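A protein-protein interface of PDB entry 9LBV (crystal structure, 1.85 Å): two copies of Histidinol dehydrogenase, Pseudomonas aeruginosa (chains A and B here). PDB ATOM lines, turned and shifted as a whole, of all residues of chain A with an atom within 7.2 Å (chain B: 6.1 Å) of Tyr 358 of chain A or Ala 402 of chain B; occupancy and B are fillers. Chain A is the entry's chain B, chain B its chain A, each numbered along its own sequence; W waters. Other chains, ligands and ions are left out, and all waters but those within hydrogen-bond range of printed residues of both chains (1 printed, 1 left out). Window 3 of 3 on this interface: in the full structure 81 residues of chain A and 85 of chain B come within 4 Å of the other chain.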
ATOM      1  N   THR A 251      11.880   2.093   7.021  1.00  0.00           N
ATOM      2  CA  THR A 251      10.505   2.520   7.276  1.00  0.00           C
ATOM      3  C   THR A 251       9.788   1.506   8.144  1.00  0.00           C
ATOM      4  O   THR A 251       9.939   0.298   7.944  1.00  0.00           O
ATOM      5  CB  THR A 251       9.707   2.707   5.972  1.00  0.00           C
ATOM      6  OG1 THR A 251      10.423   3.567   5.075  1.00  0.00           O
ATOM      7  CG2 THR A 251       8.288   3.235   6.239  1.00  0.00           C
ATOM      8  N   TRP A 255       3.624   0.626   8.500  1.00  0.00           N
ATOM      9  CA  TRP A 255       3.353   1.664   7.509  1.00  0.00           C
ATOM     10  C   TRP A 255       3.424   1.094   6.099  1.00  0.00           C
ATOM     11  O   TRP A 255       2.531   1.318   5.282  1.00  0.00           O
ATOM     12  CB  TRP A 255       4.350   2.811   7.650  1.00  0.00           C
ATOM     13  CG  TRP A 255       4.307   3.533   8.937  1.00  0.00           C
ATOM     14  CD1 TRP A 255       3.642   3.165  10.074  1.00  0.00           C
ATOM     15  CD2 TRP A 255       4.912   4.800   9.210  1.00  0.00           C
ATOM     16  NE1 TRP A 255       3.825   4.114  11.048  1.00  0.00           N
ATOM     17  CE2 TRP A 255       4.601   5.130  10.547  1.00  0.00           C
ATOM     18  CE3 TRP A 255       5.699   5.682   8.458  1.00  0.00           C
ATOM     19  CZ2 TRP A 255       5.046   6.308  11.149  1.00  0.00           C
ATOM     20  CZ3 TRP A 255       6.147   6.843   9.054  1.00  0.00           C
ATOM     21  CH2 TRP A 255       5.816   7.149  10.391  1.00  0.00           C
ATOM     22  N   GLU A 334       6.318   4.577  -4.748  1.00  0.00           N
ATOM     23  CA  GLU A 334       6.554   5.066  -3.389  1.00  0.00           C
ATOM     24  C   GLU A 334       8.009   4.773  -3.047  1.00  0.00           C
ATOM     25  O   GLU A 334       8.365   3.625  -2.763  1.00  0.00           O
ATOM     26  CB  GLU A 334       5.606   4.418  -2.387  1.00  0.00           C
ATOM     27  CG  GLU A 334       5.876   4.807  -0.945  1.00  0.00           C
ATOM     28  CD  GLU A 334       4.863   4.207   0.024  1.00  0.00           C
ATOM     29  OE1 GLU A 334       3.705   3.977  -0.378  1.00  0.00           O
ATOM     30  OE2 GLU A 334       5.212   3.992   1.196  1.00  0.00           O
ATOM     31  N   SER A 336      10.212   4.807  -0.486  1.00  0.00           N
ATOM     32  CA  SER A 336      10.252   4.899   0.977  1.00  0.00           C
ATOM     33  C   SER A 336      11.677   4.626   1.455  1.00  0.00           C
ATOM     34  O   SER A 336      11.990   3.575   2.030  1.00  0.00           O
ATOM     35  CB  SER A 336       9.245   3.936   1.607  1.00  0.00           C
ATOM     36  OG  SER A 336       9.013   4.260   2.969  1.00  0.00           O
ATOM     37  N   MET A 355       7.700  10.342  -2.014  1.00  0.00           N
ATOM     38  CA  MET A 355       9.092  10.279  -1.587  1.00  0.00           C
ATOM     39  C   MET A 355       9.205  10.293  -0.067  1.00  0.00           C
ATOM     40  O   MET A 355       8.503  11.043   0.618  1.00  0.00           O
ATOM     41  CB  MET A 355       9.914  11.438  -2.188  1.00  0.00           C
ATOM     42  CG  MET A 355      10.245  11.277  -3.680  1.00  0.00           C
ATOM     43  SD  MET A 355      11.534  12.470  -4.070  1.00  0.00           S
ATOM     44  CE  MET A 355      11.902  11.995  -5.747  1.00  0.00           C
ATOM     45  N   GLY A 356      10.088   9.462   0.455  1.00  0.00           N
ATOM     46  CA  GLY A 356      10.340   9.456   1.883  1.00  0.00           C
ATOM     47  C   GLY A 356       9.320   8.626   2.616  1.00  0.00           C
ATOM     48  O   GLY A 356       8.424   8.030   2.031  1.00  0.00           O
ATOM     49  N   ARG A 357       9.473   8.578   3.935  1.00  0.00           N
ATOM     50  CA  ARG A 357       8.658   7.719   4.784  1.00  0.00           C
ATOM     51  C   ARG A 357       7.333   8.337   5.194  1.00  0.00           C
ATOM     52  O   ARG A 357       6.417   7.602   5.584  1.00  0.00           O
ATOM     53  CB  ARG A 357       9.446   7.354   6.044  1.00  0.00           C
ATOM     54  CG  ARG A 357      10.658   6.511   5.714  1.00  0.00           C
ATOM     55  CD  ARG A 357      11.503   6.144   6.931  1.00  0.00           C
ATOM     56  NE  ARG A 357      12.928   6.365   6.693  1.00  0.00           N
ATOM     57  CZ  ARG A 357      13.656   5.672   5.823  1.00  0.00           C
ATOM     58  NH1 ARG A 357      13.120   4.738   5.040  1.00  0.00           N
ATOM     59  NH2 ARG A 357      14.959   5.909   5.739  1.00  0.00           N
ATOM     60  N   TYR A 358       7.201   9.658   5.115  1.00  0.00           N
ATOM     61  CA  TYR A 358       5.997  10.328   5.585  1.00  0.00           C
ATOM     62  C   TYR A 358       4.959  10.525   4.485  1.00  0.00           C
ATOM     63  O   TYR A 358       3.922  11.149   4.732  1.00  0.00           O
ATOM     64  CB  TYR A 358       6.363  11.682   6.197  1.00  0.00           C
ATOM     65  CG  TYR A 358       7.358  11.571   7.323  1.00  0.00           C
ATOM     66  CD1 TYR A 358       7.018  10.933   8.501  1.00  0.00           C
ATOM     67  CD2 TYR A 358       8.633  12.117   7.211  1.00  0.00           C
ATOM     68  CE1 TYR A 358       7.918  10.826   9.550  1.00  0.00           C
ATOM     69  CE2 TYR A 358       9.550  12.020   8.258  1.00  0.00           C
ATOM     70  CZ  TYR A 358       9.182  11.367   9.426  1.00  0.00           C
ATOM     71  OH  TYR A 358      10.075  11.261  10.477  1.00  0.00           O
ATOM     72  N   THR A 359       5.197  10.008   3.284  1.00  0.00           N
ATOM     73  CA  THR A 359       4.284  10.220   2.166  1.00  0.00           C
ATOM     74  C   THR A 359       3.682   8.892   1.735  1.00  0.00           C
ATOM     75  O   THR A 359       4.272   8.140   0.947  1.00  0.00           O
ATOM     76  CB  THR A 359       4.984  10.905   1.021  1.00  0.00           C
ATOM     77  OG1 THR A 359       5.616  12.076   1.536  1.00  0.00           O
ATOM     78  CG2 THR A 359       3.964  11.283  -0.050  1.00  0.00           C
ATOM     79  N   ALA A 360       2.499   8.621   2.270  1.00  0.00           N
ATOM     80  CA  ALA A 360       1.719   7.470   1.855  1.00  0.00           C
ATOM     81  C   ALA A 360       1.171   7.697   0.461  1.00  0.00           C
ATOM     82  O   ALA A 360       0.646   8.773   0.144  1.00  0.00           O
ATOM     83  CB  ALA A 360       0.571   7.239   2.838  1.00  0.00           C
ATOM     84  N   LEU A 363      -2.217   9.311  -0.001  1.00  0.00           N
ATOM     85  CA  LEU A 363      -2.409  10.752  -0.153  1.00  0.00           C
ATOM     86  C   LEU A 363      -2.574  11.151  -1.615  1.00  0.00           C
ATOM     87  O   LEU A 363      -3.228  12.160  -1.913  1.00  0.00           O
ATOM     88  CB  LEU A 363      -1.223  11.523   0.441  1.00  0.00           C
ATOM     89  CG  LEU A 363      -0.939  11.380   1.934  1.00  0.00           C
ATOM     90  CD1 LEU A 363       0.208  12.305   2.312  1.00  0.00           C
ATOM     91  CD2 LEU A 363      -2.184  11.657   2.776  1.00  0.00           C
ATOM     92  N   ASP B 117       5.698  24.211   5.827  1.00  0.00           N
ATOM     93  CA  ASP B 117       5.762  23.126   6.804  1.00  0.00           C
ATOM     94  C   ASP B 117       6.834  22.077   6.483  1.00  0.00           C
ATOM     95  O   ASP B 117       6.858  21.022   7.138  1.00  0.00           O
ATOM     96  CB  ASP B 117       4.399  22.436   6.954  1.00  0.00           C
ATOM     97  CG  ASP B 117       3.963  21.660   5.705  1.00  0.00           C
ATOM     98  OD1 ASP B 117       4.798  21.351   4.825  1.00  0.00           O
ATOM     99  OD2 ASP B 117       2.760  21.342   5.606  1.00  0.00           O
ATOM    100  N   THR B 119       7.260  20.355   3.512  1.00  0.00           N
ATOM    101  CA  THR B 119       6.921  19.479   2.392  1.00  0.00           C
ATOM    102  C   THR B 119       7.521  20.007   1.097  1.00  0.00           C
ATOM    103  O   THR B 119       7.496  21.210   0.823  1.00  0.00           O
ATOM    104  CB  THR B 119       5.396  19.348   2.270  1.00  0.00           C
ATOM    105  OG1 THR B 119       4.899  18.636   3.407  1.00  0.00           O
ATOM    106  CG2 THR B 119       4.987  18.604   0.991  1.00  0.00           C
ATOM    107  N   CYS B 400       6.351  14.684   1.658  1.00  0.00           N
ATOM    108  CA  CYS B 400       5.802  15.345   2.833  1.00  0.00           C
ATOM    109  C   CYS B 400       6.801  15.365   3.977  1.00  0.00           C
ATOM    110  O   CYS B 400       7.487  14.380   4.248  1.00  0.00           O
ATOM    111  CB  CYS B 400       4.534  14.653   3.321  1.00  0.00           C
ATOM    112  SG  CYS B 400       3.088  14.738   2.252  1.00  0.00           S
ATOM    113  N   SER B 401       6.860  16.495   4.670  1.00  0.00           N
ATOM    114  CA  SER B 401       7.395  16.474   6.018  1.00  0.00           C
ATOM    115  C   SER B 401       6.379  15.796   6.930  1.00  0.00           C
ATOM    116  O   SER B 401       5.255  15.489   6.527  1.00  0.00           O
ATOM    117  CB  SER B 401       7.703  17.891   6.491  1.00  0.00           C
ATOM    118  OG  SER B 401       6.516  18.647   6.565  1.00  0.00           O
ATOM    119  N   ALA B 402       6.788  15.530   8.172  1.00  0.00           N
ATOM    120  CA  ALA B 402       5.836  14.997   9.143  1.00  0.00           C
ATOM    121  C   ALA B 402       4.651  15.938   9.317  1.00  0.00           C
ATOM    122  O   ALA B 402       3.497  15.497   9.386  1.00  0.00           O
ATOM    123  CB  ALA B 402       6.529  14.756  10.487  1.00  0.00           C
ATOM    124  N   GLU B 403       4.920  17.244   9.379  1.00  0.00           N
ATOM    125  CA  GLU B 403       3.836  18.209   9.532  1.00  0.00           C
ATOM    126  C   GLU B 403       2.943  18.230   8.296  1.00  0.00           C
ATOM    127  O   GLU B 403       1.713  18.246   8.415  1.00  0.00           O
ATOM    128  CB  GLU B 403       4.409  19.604   9.802  1.00  0.00           C
ATOM    129  CG  GLU B 403       3.358  20.671  10.084  1.00  0.00           C
ATOM    130  CD  GLU B 403       2.297  20.215  11.093  1.00  0.00           C
ATOM    131  OE1 GLU B 403       2.666  19.556  12.092  1.00  0.00           O
ATOM    132  OE2 GLU B 403       1.094  20.509  10.888  1.00  0.00           O
ATOM    133  N   GLY B 404       3.543  18.231   7.101  1.00  0.00           N
ATOM    134  CA  GLY B 404       2.736  18.221   5.883  1.00  0.00           C
ATOM    135  C   GLY B 404       1.866  16.981   5.761  1.00  0.00           C
ATOM    136  O   GLY B 404       0.704  17.061   5.338  1.00  0.00           O
ATOM    137  N   ALA B 405       2.408  15.816   6.139  1.00  0.00           N
ATOM    138  CA  ALA B 405       1.616  14.591   6.102  1.00  0.00           C
ATOM    139  C   ALA B 405       0.457  14.649   7.082  1.00  0.00           C
ATOM    140  O   ALA B 405      -0.590  14.029   6.840  1.00  0.00           O
ATOM    141  CB  ALA B 405       2.498  13.375   6.396  1.00  0.00           C
ATOM    142  N   SER B 406       0.622  15.378   8.197  1.00  0.00           N
ATOM    143  CA  SER B 406      -0.481  15.527   9.149  1.00  0.00           C
ATOM    144  C   SER B 406      -1.615  16.339   8.540  1.00  0.00           C
ATOM    145  O   SER B 406      -2.781  15.947   8.607  1.00  0.00           O
ATOM    146  CB  SER B 406       0.005  16.202  10.440  1.00  0.00           C
ATOM    147  OG  SER B 406       1.055  15.484  11.047  1.00  0.00           O
ATOM    148  N   VAL B 407      -1.282  17.492   7.957  1.00  0.00           N
ATOM    149  CA  VAL B 407      -2.285  18.334   7.313  1.00  0.00           C
ATOM    150  C   VAL B 407      -3.017  17.547   6.233  1.00  0.00           C
ATOM    151  O   VAL B 407      -4.246  17.441   6.249  1.00  0.00           O
ATOM    152  CB  VAL B 407      -1.628  19.600   6.735  1.00  0.00           C
ATOM    153  CG1 VAL B 407      -2.629  20.409   5.910  1.00  0.00           C
ATOM    154  CG2 VAL B 407      -1.024  20.432   7.844  1.00  0.00           C
ATOM    155  N   ARG B 431       1.089   8.671   9.851  1.00  0.00           N
ATOM    156  CA  ARG B 431       1.962   9.846   9.805  1.00  0.00           C
ATOM    157  C   ARG B 431       1.343  11.110  10.380  1.00  0.00           C
ATOM    158  O   ARG B 431       2.015  12.151  10.401  1.00  0.00           O
ATOM    159  CB  ARG B 431       2.448  10.068   8.355  1.00  0.00           C
ATOM    160  CG  ARG B 431       3.291   8.857   7.963  1.00  0.00           C
ATOM    161  CD  ARG B 431       2.658   7.731   7.198  1.00  0.00           C
ATOM    162  NE  ARG B 431       3.621   7.128   6.284  1.00  0.00           N
ATOM    163  CZ  ARG B 431       3.347   6.110   5.479  1.00  0.00           C
ATOM    164  NH1 ARG B 431       2.133   5.597   5.407  1.00  0.00           N
ATOM    165  NH2 ARG B 431       4.327   5.571   4.759  1.00  0.00           N
ATOM    166  N   ILE B 432       0.094  11.055  10.842  1.00  0.00           N
ATOM    167  CA  ILE B 432      -0.535  12.218  11.463  1.00  0.00           C
ATOM    168  C   ILE B 432       0.036  12.409  12.865  1.00  0.00           C
ATOM    169  O   ILE B 432      -0.044  11.510  13.709  1.00  0.00           O
ATOM    170  CB  ILE B 432      -2.061  12.059  11.514  1.00  0.00           C
ATOM    171  CG1 ILE B 432      -2.647  11.893  10.106  1.00  0.00           C
ATOM    172  CG2 ILE B 432      -2.682  13.277  12.189  1.00  0.00           C
ATOM    173  CD1 ILE B 432      -4.190  11.729  10.073  1.00  0.00           C
ATOM    174  N   LEU B 433       0.601  13.587  13.123  1.00  0.00           N
ATOM    175  CA  LEU B 433       0.997  13.974  14.473  1.00  0.00           C
ATOM    176  C   LEU B 433      -0.229  14.385  15.284  1.00  0.00           C
ATOM    177  O   LEU B 433      -1.194  14.945  14.751  1.00  0.00           O
ATOM    178  CB  LEU B 433       1.992  15.138  14.430  1.00  0.00           C
ATOM    179  CG  LEU B 433       3.206  14.897  13.540  1.00  0.00           C
ATOM    180  CD1 LEU B 433       4.063  16.167  13.389  1.00  0.00           C
ATOM    181  CD2 LEU B 433       4.011  13.729  14.088  1.00  0.00           C
HETATM  182  O   HOH W   1       7.852  11.907   3.002  1.00  0.00           O
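N of Cys 400 of chain B lies within hydrogen-bond range of OG1 of Thr 359 of chain A (2.7 Å).
The side-chain carboxylate (OE2) of Glu 334 of chain A is in salt-bridge range of the guanidinium group (NH2) of Arg 431 of chain B (3.996 Å).
NE of Arg 431 of chain B sits at hydrogen-bond distance from O of Arg 357 of chain A.
N of Ser 401 of chain B lies within hydrogen-bond range of OG1 of Thr 119 of chain B, 3.2 Å away.
OG of Ser 401 of chain B lies within hydrogen-bond range of N of Gly 404 of chain B (3.0 Å).
The side-chain hydroxyl of Ser 406 of chain B is in hydrogen-bond range of the backbone carbonyl oxygen of Ala 402 of chain B, 3.0 Å away.
OG1 of Thr 251 of chain A sits at hydrogen-bond distance from NH1 of Arg 357 of chain A.
NH1 of Arg 357 of chain A sits at hydrogen-bond distance from O of Ser 336 of chain A (3.4 Å).
O of Met 355 of chain A sits at hydrogen-bond distance from OG1 of Thr 359 of chain A.
Among the printed residues, merely in contact across the chains: Trp 255 of chain A with Arg 431 of chain B (3.3 Å), Tyr 358 of chain A with Cys 400 of chain B (3.5 Å), Tyr 358 of chain A with Ser 401 of chain B (3.98 Å), Tyr 358 of chain A with Ala 402 of chain B (3.997 Å), Tyr 358 of chain A with Ala 405 of chain B (3.1 Å), Tyr 358 of chain A with Arg 431 of chain B (3.9 Å), Ala 360 of chain A with Arg 431 of chain B (3.4 Å) and Leu 363 of chain A with Cys 400 of chain B (3.8 Å).
Of the printed residues of chain B, Tyr 358 of chain A touches Cys 400 (3.5 Å), Ser 401 (3.98 Å), Ala 402 (3.997 Å), Ala 405 (3.1 Å) and Arg 431 (3.9 Å).
Of the printed residues of chain A, Ala 402 of chain B touches Tyr 358.
Printed residues of chain B within 4 Å of Leu 363 of chain A: Cys 400.
Of the printed residues of chain A, Arg 431 of chain B touches Trp 255 (3.3 Å), Glu 334 (3.996 Å), Arg 357 (2.9 Å), Tyr 358 (3.9 Å) and Ala 360 (3.4 Å).
Of the printed residues of chain A, Ala 405 of chain B touches Tyr 358 (3.1 Å).
Printed residues of chain B within 4 Å of Trp 255 of chain A: Arg 431 (3.3 Å).
Of the printed residues of chain B, Arg 357 of chain A touches Arg 431.
The nearest printed residue of chain B that does not touch Tyr 358 of chain A is Gly 404 of chain B (6.3 Å).
The nearest printed residue of chain A that does not touch Ala 402 of chain B is Thr 359 of chain A (7.5 Å).
Of the 11 printed residues of chain A, 7 touch a printed residue of chain B.
Hydrophobic or aromatic side chains of chain A within 4 Å of the printed part of chain B: Trp 255, Tyr 358, Ala 360 and Leu 363.
Hydrophobic or aromatic side chains of chain B that line the printed part of chain A: Ala 405.
Among the printed residues, 11 pairs touch across the chains.
Among the printed residues, Asp or Glu carboxylates within 4 Å of a Lys or Arg side-chain nitrogen of the other chain: Glu 334 of chain A with Arg 431 of chain B.
No position is printed for both chains.
Of the 11 pairs that touch across the chains among the printed residues, none has its exchanged pair printed and touching as well.
Water W1 lies within hydrogen-bond range of O of Met 355 of chain A, OG1 of Thr 359 of chain A, O of Cys 400 of chain B and N of Tyr 358 of chain A.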
